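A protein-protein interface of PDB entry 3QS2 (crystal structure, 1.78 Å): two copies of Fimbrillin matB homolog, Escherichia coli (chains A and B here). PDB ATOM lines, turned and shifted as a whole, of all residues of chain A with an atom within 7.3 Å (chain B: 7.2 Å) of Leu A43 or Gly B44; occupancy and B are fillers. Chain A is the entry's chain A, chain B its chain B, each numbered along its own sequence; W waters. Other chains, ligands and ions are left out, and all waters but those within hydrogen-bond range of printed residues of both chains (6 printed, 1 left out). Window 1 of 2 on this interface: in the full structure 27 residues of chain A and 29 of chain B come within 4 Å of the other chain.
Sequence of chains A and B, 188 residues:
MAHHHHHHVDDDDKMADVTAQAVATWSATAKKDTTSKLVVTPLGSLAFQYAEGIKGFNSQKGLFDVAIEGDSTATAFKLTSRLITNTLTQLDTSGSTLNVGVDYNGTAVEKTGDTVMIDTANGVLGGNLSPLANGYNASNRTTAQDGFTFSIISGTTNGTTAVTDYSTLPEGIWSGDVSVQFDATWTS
The backbone NH of Thr A41 sits at hydrogen-bond distance from the backbone carbonyl oxygen of Asp B65 (2.8 Å).
N of Leu A43 lies within hydrogen-bond range of O of Leu B63 (2.9 Å).
The backbone NH (N) of Leu B43 is in hydrogen-bond range of the backbone carbonyl oxygen (O) of Leu A63, 2.9 Å away.
O of Asp A65 is in hydrogen-bond range of N of Thr B41 (2.8 Å).
The side-chain hydroxyl of Ser A45 lies within hydrogen-bond range of the backbone carbonyl oxygen of Pro A42 (2.8 Å).
The side-chain hydroxyl (OG) of Ser B45 is in hydrogen-bond range of the backbone carbonyl oxygen (O) of Pro B42 (2.8 Å).
The backbone carbonyl oxygen (O) of Asp B146 is in hydrogen-bond range of the backbone NH (N) of Phe B64, 2.8 Å away.
OD1 of Asp B65 sits at hydrogen-bond distance from NE2 of Gln B145.
Among the printed residues, merely in contact across the chains: Trp A26 with Pro B42 (3.5 Å), Thr A41 with Phe B64 (3.4 Å), Pro A42 with Thr B25 (3.5 Å), Pro A42 with Trp B26 (3.6 Å), Pro A42 with Leu B63 (3.6 Å), Leu A43 with Gly B44 (3.4 Å), Leu A43 with Phe B64 (3.8 Å), Leu A43 with Asp B65 (3.7 Å), Leu A43 with Gln B145 (3.6 Å), Gly A44 with Leu B43 (3.5 Å), Leu A63 with Pro B42 (3.5 Å) and Asp A65 with Leu B43 (3.5 Å).
Leu A43 touches just these residues of chain B: Gly B44 (3.4 Å), Leu B63 (2.9 Å), Phe B64 (3.8 Å), Asp B65 (3.7 Å) and Gln B145 (3.6 Å).
Gly B44 touches just one residue of chain A: Leu A43 (3.4 Å).
Printed residues of chain B within 4 Å of Leu A63: Pro B42 and Leu B43.
Of the printed residues of chain A, Leu B63 touches Pro A42 and Leu A43.
The nearest residue of chain A that does not touch Gly B44 is Gly A44 (4.5 Å).
Hydrophobic or aromatic side chains of chain B that line the printed part of chain A: Trp B26, Pro B42, Leu B43, Leu B63 and Phe B64.
Printed residues of chain A that touch a printed residue of chain B: Trp A26, Thr A41, Pro A42, Leu A43, Gly A44, Leu A63 and Asp A65.
Hydrophobic or aromatic side chains of chain A that line the printed part of chain B: Trp A26, Pro A42, Leu A43 and Leu A63.
Among the printed residues, no Asp or Glu carboxylate lies within 4 Å of a Lys or Arg side-chain nitrogen of the other chain.
Pro A42 touches Leu B63, and with the chains exchanged Leu A63 touches Pro B42.
Leu A43 touches Gly B44, and with the chains exchanged Gly A44 touches Leu B43.
Leu A43 touches Leu B63, and with the chains exchanged Leu A63 touches Leu B43.
Leu A43 touches Asp B65, and with the chains exchanged Asp A65 touches Leu B43.
Water W5 lies within hydrogen-bond range of the backbone carbonyl oxygen of Gly A44, the backbone carbonyl oxygen of Leu B43 and the indole nitrogen of Trp A26.
Water W1 lies within hydrogen-bond range of O of Leu A43, N of Ser A45 and O of Gly B44.
Water W2 bridges the backbone carbonyl oxygen (O) of Leu B43 (2.9 Å) and the backbone carbonyl oxygen (O) of Gly A44 (3.0 Å).
Water W6 lies within hydrogen-bond range of the backbone carbonyl oxygen (O) of Thr A41 (3.0 Å) and the side-chain carboxylate (OD2) of Asp B65 (3.1 Å).
Water W3 bridges OG1 of Thr B41 (3.0 Å) and O of Asp A65 (3.1 Å).
Water W4 bridges OG1 of Thr A41 (3.1 Å) and O of Asp B65 (3.3 Å).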
ATOM      1  N   TRP A  26     -37.815 -32.971  29.991  1.00  0.00           N
ATOM      2  CA  TRP A  26     -37.340 -32.228  28.822  1.00  0.00           C
ATOM      3  C   TRP A  26     -38.312 -31.107  28.525  1.00  0.00           C
ATOM      4  O   TRP A  26     -39.526 -31.309  28.577  1.00  0.00           O
ATOM      5  CB  TRP A  26     -37.353 -33.119  27.561  1.00  0.00           C
ATOM      6  CG  TRP A  26     -36.233 -34.149  27.448  1.00  0.00           C
ATOM      7  CD1 TRP A  26     -35.082 -34.019  26.727  1.00  0.00           C
ATOM      8  CD2 TRP A  26     -36.175 -35.454  28.066  1.00  0.00           C
ATOM      9  NE1 TRP A  26     -34.308 -35.148  26.859  1.00  0.00           N
ATOM     10  CE2 TRP A  26     -34.946 -36.041  27.677  1.00  0.00           C
ATOM     11  CE3 TRP A  26     -37.043 -36.181  28.894  1.00  0.00           C
ATOM     12  CZ2 TRP A  26     -34.558 -37.331  28.080  1.00  0.00           C
ATOM     13  CZ3 TRP A  26     -36.638 -37.465  29.327  1.00  0.00           C
ATOM     14  CH2 TRP A  26     -35.417 -38.018  28.908  1.00  0.00           C
ATOM     15  N   THR A  41     -32.713 -22.165  19.902  1.00  0.00           N
ATOM     16  CA  THR A  41     -32.934 -23.516  20.379  1.00  0.00           C
ATOM     17  C   THR A  41     -31.940 -23.932  21.456  1.00  0.00           C
ATOM     18  O   THR A  41     -30.775 -24.127  21.152  1.00  0.00           O
ATOM     19  CB  THR A  41     -32.777 -24.512  19.215  1.00  0.00           C
ATOM     20  OG1 THR A  41     -33.581 -24.079  18.101  1.00  0.00           O
ATOM     21  CG2 THR A  41     -33.204 -25.891  19.663  1.00  0.00           C
ATOM     22  N   PRO A  42     -32.405 -24.095  22.720  1.00  0.00           N
ATOM     23  CA  PRO A  42     -31.496 -24.594  23.742  1.00  0.00           C
ATOM     24  C   PRO A  42     -30.965 -25.986  23.382  1.00  0.00           C
ATOM     25  O   PRO A  42     -31.745 -26.821  22.916  1.00  0.00           O
ATOM     26  CB  PRO A  42     -32.403 -24.736  24.977  1.00  0.00           C
ATOM     27  CG  PRO A  42     -33.462 -23.702  24.781  1.00  0.00           C
ATOM     28  CD  PRO A  42     -33.744 -23.788  23.277  1.00  0.00           C
ATOM     29  N   LEU A  43     -29.685 -26.252  23.605  1.00  0.00           N
ATOM     30  CA  LEU A  43     -29.157 -27.563  23.267  1.00  0.00           C
ATOM     31  C   LEU A  43     -29.874 -28.600  24.120  1.00  0.00           C
ATOM     32  O   LEU A  43     -30.052 -28.408  25.320  1.00  0.00           O
ATOM     33  CB  LEU A  43     -27.644 -27.636  23.467  1.00  0.00           C
ATOM     34  CG  LEU A  43     -26.784 -27.319  22.239  1.00  0.00           C
ATOM     35  CD1 LEU A  43     -26.980 -25.901  21.732  1.00  0.00           C
ATOM     36  CD2 LEU A  43     -25.328 -27.559  22.555  1.00  0.00           C
ATOM     37  N   GLY A  44     -30.299 -29.687  23.487  1.00  0.00           N
ATOM     38  CA  GLY A  44     -30.935 -30.765  24.208  1.00  0.00           C
ATOM     39  C   GLY A  44     -32.433 -30.631  24.202  1.00  0.00           C
ATOM     40  O   GLY A  44     -33.141 -31.553  24.614  1.00  0.00           O
ATOM     41  N   SER A  45     -32.935 -29.473  23.772  1.00  0.00           N
ATOM     42  CA  SER A  45     -34.385 -29.262  23.799  1.00  0.00           C
ATOM     43  C   SER A  45     -35.034 -30.029  22.667  1.00  0.00           C
ATOM     44  O   SER A  45     -34.402 -30.324  21.631  1.00  0.00           O
ATOM     45  CB  SER A  45     -34.731 -27.771  23.723  1.00  0.00           C
ATOM     46  OG  SER A  45     -34.485 -27.292  22.418  1.00  0.00           O
ATOM     47  N   LEU A  46     -36.306 -30.371  22.869  1.00  0.00           N
ATOM     48  CA  LEU A  46     -37.064 -31.089  21.875  1.00  0.00           C
ATOM     49  C   LEU A  46     -37.737 -30.023  21.033  1.00  0.00           C
ATOM     50  O   LEU A  46     -38.484 -29.207  21.568  1.00  0.00           O
ATOM     51  CB  LEU A  46     -38.110 -31.982  22.547  1.00  0.00           C
ATOM     52  CG  LEU A  46     -37.547 -32.956  23.573  1.00  0.00           C
ATOM     53  CD1 LEU A  46     -38.667 -33.808  24.172  1.00  0.00           C
ATOM     54  CD2 LEU A  46     -36.485 -33.830  22.913  1.00  0.00           C
ATOM     55  N   LEU A  63     -31.613 -37.327  24.583  1.00  0.00           N
ATOM     56  CA  LEU A  63     -30.708 -38.165  25.361  1.00  0.00           C
ATOM     57  C   LEU A  63     -30.779 -37.914  26.866  1.00  0.00           C
ATOM     58  O   LEU A  63     -31.165 -36.829  27.314  1.00  0.00           O
ATOM     59  CB  LEU A  63     -29.254 -38.016  24.886  1.00  0.00           C
ATOM     60  CG  LEU A  63     -28.927 -38.278  23.415  1.00  0.00           C
ATOM     61  CD1 LEU A  63     -27.404 -38.107  23.147  1.00  0.00           C
ATOM     62  CD2 LEU A  63     -29.423 -39.642  23.007  1.00  0.00           C
ATOM     63  N   ASP A  65     -28.664 -39.108  30.814  1.00  0.00           N
ATOM     64  CA  ASP A  65     -27.612 -39.787  31.551  1.00  0.00           C
ATOM     65  C   ASP A  65     -28.237 -40.439  32.755  1.00  0.00           C
ATOM     66  O   ASP A  65     -29.168 -39.882  33.355  1.00  0.00           O
ATOM     67  CB  ASP A  65     -26.567 -38.769  31.989  1.00  0.00           C
ATOM     68  CG  ASP A  65     -25.815 -38.188  30.816  1.00  0.00           C
ATOM     69  OD1 ASP A  65     -25.513 -38.937  29.872  1.00  0.00           O
ATOM     70  OD2 ASP A  65     -25.489 -36.993  30.841  1.00  0.00           O
ATOM     71  N   THR B  25     -36.525 -22.070  26.121  1.00  0.00           N
ATOM     72  CA  THR B  25     -36.880 -22.548  27.453  1.00  0.00           C
ATOM     73  C   THR B  25     -36.025 -23.758  27.822  1.00  0.00           C
ATOM     74  O   THR B  25     -35.935 -24.689  27.041  1.00  0.00           O
ATOM     75  CB  THR B  25     -38.361 -22.944  27.520  1.00  0.00           C
ATOM     76  OG1 THR B  25     -39.174 -21.852  27.080  1.00  0.00           O
ATOM     77  CG2 THR B  25     -38.750 -23.399  28.953  1.00  0.00           C
ATOM     78  N   TRP B  26     -35.427 -23.718  29.015  1.00  0.00           N
ATOM     79  CA  TRP B  26     -34.695 -24.843  29.586  1.00  0.00           C
ATOM     80  C   TRP B  26     -35.541 -25.438  30.723  1.00  0.00           C
ATOM     81  O   TRP B  26     -36.136 -24.716  31.508  1.00  0.00           O
ATOM     82  CB  TRP B  26     -33.383 -24.365  30.215  1.00  0.00           C
ATOM     83  CG  TRP B  26     -32.288 -24.046  29.228  1.00  0.00           C
ATOM     84  CD1 TRP B  26     -31.262 -24.856  28.890  1.00  0.00           C
ATOM     85  CD2 TRP B  26     -32.104 -22.818  28.495  1.00  0.00           C
ATOM     86  NE1 TRP B  26     -30.448 -24.234  27.986  1.00  0.00           N
ATOM     87  CE2 TRP B  26     -30.941 -22.979  27.720  1.00  0.00           C
ATOM     88  CE3 TRP B  26     -32.824 -21.599  28.410  1.00  0.00           C
ATOM     89  CZ2 TRP B  26     -30.459 -21.980  26.861  1.00  0.00           C
ATOM     90  CZ3 TRP B  26     -32.346 -20.598  27.555  1.00  0.00           C
ATOM     91  CH2 TRP B  26     -31.178 -20.797  26.787  1.00  0.00           C
ATOM     92  N   SER B  27     -35.588 -26.758  30.818  1.00  0.00           N
ATOM     93  CA  SER B  27     -36.131 -27.408  32.008  1.00  0.00           C
ATOM     94  C   SER B  27     -35.010 -27.407  33.059  1.00  0.00           C
ATOM     95  O   SER B  27     -33.837 -27.669  32.728  1.00  0.00           O
ATOM     96  CB  SER B  27     -36.589 -28.825  31.667  1.00  0.00           C
ATOM     97  OG  SER B  27     -36.726 -29.635  32.823  1.00  0.00           O
ATOM     98  N   THR B  41     -30.692 -37.609  34.144  1.00  0.00           N
ATOM     99  CA  THR B  41     -30.508 -36.211  33.776  1.00  0.00           C
ATOM    100  C   THR B  41     -30.646 -36.060  32.268  1.00  0.00           C
ATOM    101  O   THR B  41     -29.797 -36.553  31.538  1.00  0.00           O
ATOM    102  CB  THR B  41     -29.114 -35.736  34.177  1.00  0.00           C
ATOM    103  OG1 THR B  41     -28.892 -36.052  35.556  1.00  0.00           O
ATOM    104  CG2 THR B  41     -29.025 -34.214  34.008  1.00  0.00           C
ATOM    105  N   PRO B  42     -31.700 -35.367  31.793  1.00  0.00           N
ATOM    106  CA  PRO B  42     -31.762 -35.136  30.351  1.00  0.00           C
ATOM    107  C   PRO B  42     -30.593 -34.273  29.889  1.00  0.00           C
ATOM    108  O   PRO B  42     -30.254 -33.304  30.561  1.00  0.00           O
ATOM    109  CB  PRO B  42     -33.088 -34.358  30.174  1.00  0.00           C
ATOM    110  CG  PRO B  42     -33.909 -34.743  31.364  1.00  0.00           C
ATOM    111  CD  PRO B  42     -32.885 -34.835  32.483  1.00  0.00           C
ATOM    112  N   LEU B  43     -29.972 -34.615  28.766  1.00  0.00           N
ATOM    113  CA  LEU B  43     -28.884 -33.778  28.246  1.00  0.00           C
ATOM    114  C   LEU B  43     -29.359 -32.373  27.940  1.00  0.00           C
ATOM    115  O   LEU B  43     -30.408 -32.184  27.310  1.00  0.00           O
ATOM    116  CB  LEU B  43     -28.272 -34.386  26.995  1.00  0.00           C
ATOM    117  CG  LEU B  43     -27.068 -35.264  27.307  1.00  0.00           C
ATOM    118  CD1 LEU B  43     -27.531 -36.496  28.073  1.00  0.00           C
ATOM    119  CD2 LEU B  43     -26.331 -35.660  26.008  1.00  0.00           C
ATOM    120  N   GLY B  44     -28.586 -31.389  28.390  1.00  0.00           N
ATOM    121  CA  GLY B  44     -28.911 -30.002  28.098  1.00  0.00           C
ATOM    122  C   GLY B  44     -29.793 -29.373  29.155  1.00  0.00           C
ATOM    123  O   GLY B  44     -29.937 -28.164  29.183  1.00  0.00           O
ATOM    124  N   SER B  45     -30.408 -30.182  30.025  1.00  0.00           N
ATOM    125  CA  SER B  45     -31.195 -29.621  31.121  1.00  0.00           C
ATOM    126  C   SER B  45     -30.289 -28.980  32.172  1.00  0.00           C
ATOM    127  O   SER B  45     -29.129 -29.367  32.347  1.00  0.00           O
ATOM    128  CB  SER B  45     -32.068 -30.684  31.772  1.00  0.00           C
ATOM    129  OG  SER B  45     -31.276 -31.598  32.521  1.00  0.00           O
ATOM    130  N   LEU B  46     -30.830 -28.004  32.884  1.00  0.00           N
ATOM    131  CA  LEU B  46     -30.068 -27.317  33.918  1.00  0.00           C
ATOM    132  C   LEU B  46     -30.249 -28.111  35.193  1.00  0.00           C
ATOM    133  O   LEU B  46     -31.366 -28.478  35.520  1.00  0.00           O
ATOM    134  CB  LEU B  46     -30.596 -25.889  34.094  1.00  0.00           C
ATOM    135  CG  LEU B  46     -30.535 -25.045  32.824  1.00  0.00           C
ATOM    136  CD1 LEU B  46     -31.262 -23.721  33.018  1.00  0.00           C
ATOM    137  CD2 LEU B  46     -29.087 -24.811  32.408  1.00  0.00           C
ATOM    138  N   ALA B  47     -29.138 -28.405  35.861  1.00  0.00           N
ATOM    139  CA  ALA B  47     -29.132 -29.202  37.086  1.00  0.00           C
ATOM    140  C   ALA B  47     -28.298 -28.520  38.164  1.00  0.00           C
ATOM    141  O   ALA B  47     -27.100 -28.260  37.984  1.00  0.00           O
ATOM    142  CB  ALA B  47     -28.610 -30.602  36.789  1.00  0.00           C
ATOM    143  N   GLN B  60     -24.203 -23.334  35.931  1.00  0.00           N
ATOM    144  CA  GLN B  60     -24.087 -24.189  34.756  1.00  0.00           C
ATOM    145  C   GLN B  60     -24.224 -23.327  33.521  1.00  0.00           C
ATOM    146  O   GLN B  60     -25.115 -22.480  33.470  1.00  0.00           O
ATOM    147  CB  GLN B  60     -25.175 -25.271  34.779  1.00  0.00           C
ATOM    148  CG  GLN B  60     -25.083 -26.263  33.597  1.00  0.00           C
ATOM    149  CD  GLN B  60     -26.181 -27.315  33.616  1.00  0.00           C
ATOM    150  OE1 GLN B  60     -26.643 -27.721  34.676  1.00  0.00           O
ATOM    151  NE2 GLN B  60     -26.601 -27.753  32.438  1.00  0.00           N
ATOM    152  N   LYS B  61     -23.347 -23.517  32.536  1.00  0.00           N
ATOM    153  CA  LYS B  61     -23.520 -22.804  31.275  1.00  0.00           C
ATOM    154  C   LYS B  61     -24.456 -23.620  30.400  1.00  0.00           C
ATOM    155  O   LYS B  61     -24.142 -24.765  30.042  1.00  0.00           O
ATOM    156  CB  LYS B  61     -22.164 -22.566  30.592  1.00  0.00           C
ATOM    157  CG  LYS B  61     -22.269 -21.688  29.370  1.00  0.00           C
ATOM    158  CD  LYS B  61     -20.883 -21.312  28.875  1.00  0.00           C
ATOM    159  CE  LYS B  61     -20.992 -20.376  27.706  1.00  0.00           C
ATOM    160  NZ  LYS B  61     -19.627 -19.899  27.312  1.00  0.00           N
ATOM    161  N   GLY B  62     -25.614 -23.039  30.081  1.00  0.00           N
ATOM    162  CA  GLY B  62     -26.582 -23.659  29.152  1.00  0.00           C
ATOM    163  C   GLY B  62     -26.416 -23.073  27.758  1.00  0.00           C
ATOM    164  O   GLY B  62     -26.504 -21.855  27.579  1.00  0.00           O
ATOM    165  N   LEU B  63     -26.158 -23.940  26.775  1.00  0.00           N
ATOM    166  CA  LEU B  63     -25.870 -23.475  25.404  1.00  0.00           C
ATOM    167  C   LEU B  63     -27.152 -23.403  24.583  1.00  0.00           C
ATOM    168  O   LEU B  63     -28.127 -24.106  24.868  1.00  0.00           O
ATOM    169  CB  LEU B  63     -24.870 -24.394  24.711  1.00  0.00           C
ATOM    170  CG  LEU B  63     -23.560 -24.638  25.462  1.00  0.00           C
ATOM    171  CD1 LEU B  63     -22.683 -25.532  24.623  1.00  0.00           C
ATOM    172  CD2 LEU B  63     -22.884 -23.292  25.719  1.00  0.00           C
ATOM    173  N   PHE B  64     -27.139 -22.540  23.569  1.00  0.00           N
ATOM    174  CA  PHE B  64     -28.247 -22.416  22.613  1.00  0.00           C
ATOM    175  C   PHE B  64     -27.706 -22.112  21.234  1.00  0.00           C
ATOM    176  O   PHE B  64     -26.606 -21.553  21.087  1.00  0.00           O
ATOM    177  CB  PHE B  64     -29.227 -21.305  23.035  1.00  0.00           C
ATOM    178  CG  PHE B  64     -28.563 -19.980  23.314  1.00  0.00           C
ATOM    179  CD1 PHE B  64     -28.330 -19.073  22.283  1.00  0.00           C
ATOM    180  CD2 PHE B  64     -28.163 -19.652  24.606  1.00  0.00           C
ATOM    181  CE1 PHE B  64     -27.712 -17.847  22.525  1.00  0.00           C
ATOM    182  CE2 PHE B  64     -27.542 -18.419  24.859  1.00  0.00           C
ATOM    183  CZ  PHE B  64     -27.316 -17.531  23.823  1.00  0.00           C
ATOM    184  N   ASP B  65     -28.481 -22.482  20.213  1.00  0.00           N
ATOM    185  CA  ASP B  65     -28.170 -22.114  18.832  1.00  0.00           C
ATOM    186  C   ASP B  65     -29.149 -21.052  18.380  1.00  0.00           C
ATOM    187  O   ASP B  65     -30.336 -21.123  18.734  1.00  0.00           O
ATOM    188  CB  ASP B  65     -28.321 -23.316  17.910  1.00  0.00           C
ATOM    189  CG  ASP B  65     -27.292 -24.384  18.179  1.00  0.00           C
ATOM    190  OD1 ASP B  65     -26.143 -24.020  18.494  1.00  0.00           O
ATOM    191  OD2 ASP B  65     -27.645 -25.588  18.077  1.00  0.00           O
ATOM    192  N   GLN B 145     -23.694 -20.360  17.821  1.00  0.00           N
ATOM    193  CA  GLN B 145     -23.964 -20.933  19.139  1.00  0.00           C
ATOM    194  C   GLN B 145     -23.341 -20.074  20.227  1.00  0.00           C
ATOM    195  O   GLN B 145     -22.241 -19.543  20.060  1.00  0.00           O
ATOM    196  CB  GLN B 145     -23.361 -22.333  19.208  1.00  0.00           C
ATOM    197  CG  GLN B 145     -23.680 -23.125  20.486  1.00  0.00           C
ATOM    198  CD  GLN B 145     -23.229 -24.560  20.336  1.00  0.00           C
ATOM    199  OE1 GLN B 145     -22.125 -24.913  20.758  1.00  0.00           O
ATOM    200  NE2 GLN B 145     -24.050 -25.383  19.671  1.00  0.00           N
ATOM    201  N   ASP B 146     -24.046 -19.964  21.352  1.00  0.00           N
ATOM    202  CA  ASP B 146     -23.499 -19.302  22.522  1.00  0.00           C
ATOM    203  C   ASP B 146     -24.177 -19.903  23.755  1.00  0.00           C
ATOM    204  O   ASP B 146     -24.792 -20.956  23.662  1.00  0.00           O
ATOM    205  CB  ASP B 146     -23.683 -17.779  22.452  1.00  0.00           C
ATOM    206  CG  ASP B 146     -22.542 -17.029  23.138  1.00  0.00           C
ATOM    207  OD1 ASP B 146     -21.897 -17.588  24.056  1.00  0.00           O
ATOM    208  OD2 ASP B 146     -22.293 -15.860  22.790  1.00  0.00           O
HETATM  209  O   HOH W   1     -32.292 -28.400  26.782  1.00  0.00           O
HETATM  210  O   HOH W   2     -32.977 -30.916  27.553  1.00  0.00           O
HETATM  211  O   HOH W   3     -27.449 -38.639  35.547  1.00  0.00           O
HETATM  212  O   HOH W   4     -31.718 -22.615  16.155  1.00  0.00           O
HETATM  213  O   HOH W   5     -32.014 -33.756  25.627  1.00  0.00           O
HETATM  214  O   HOH W   6     -29.982 -26.620  19.788  1.00  0.00           O
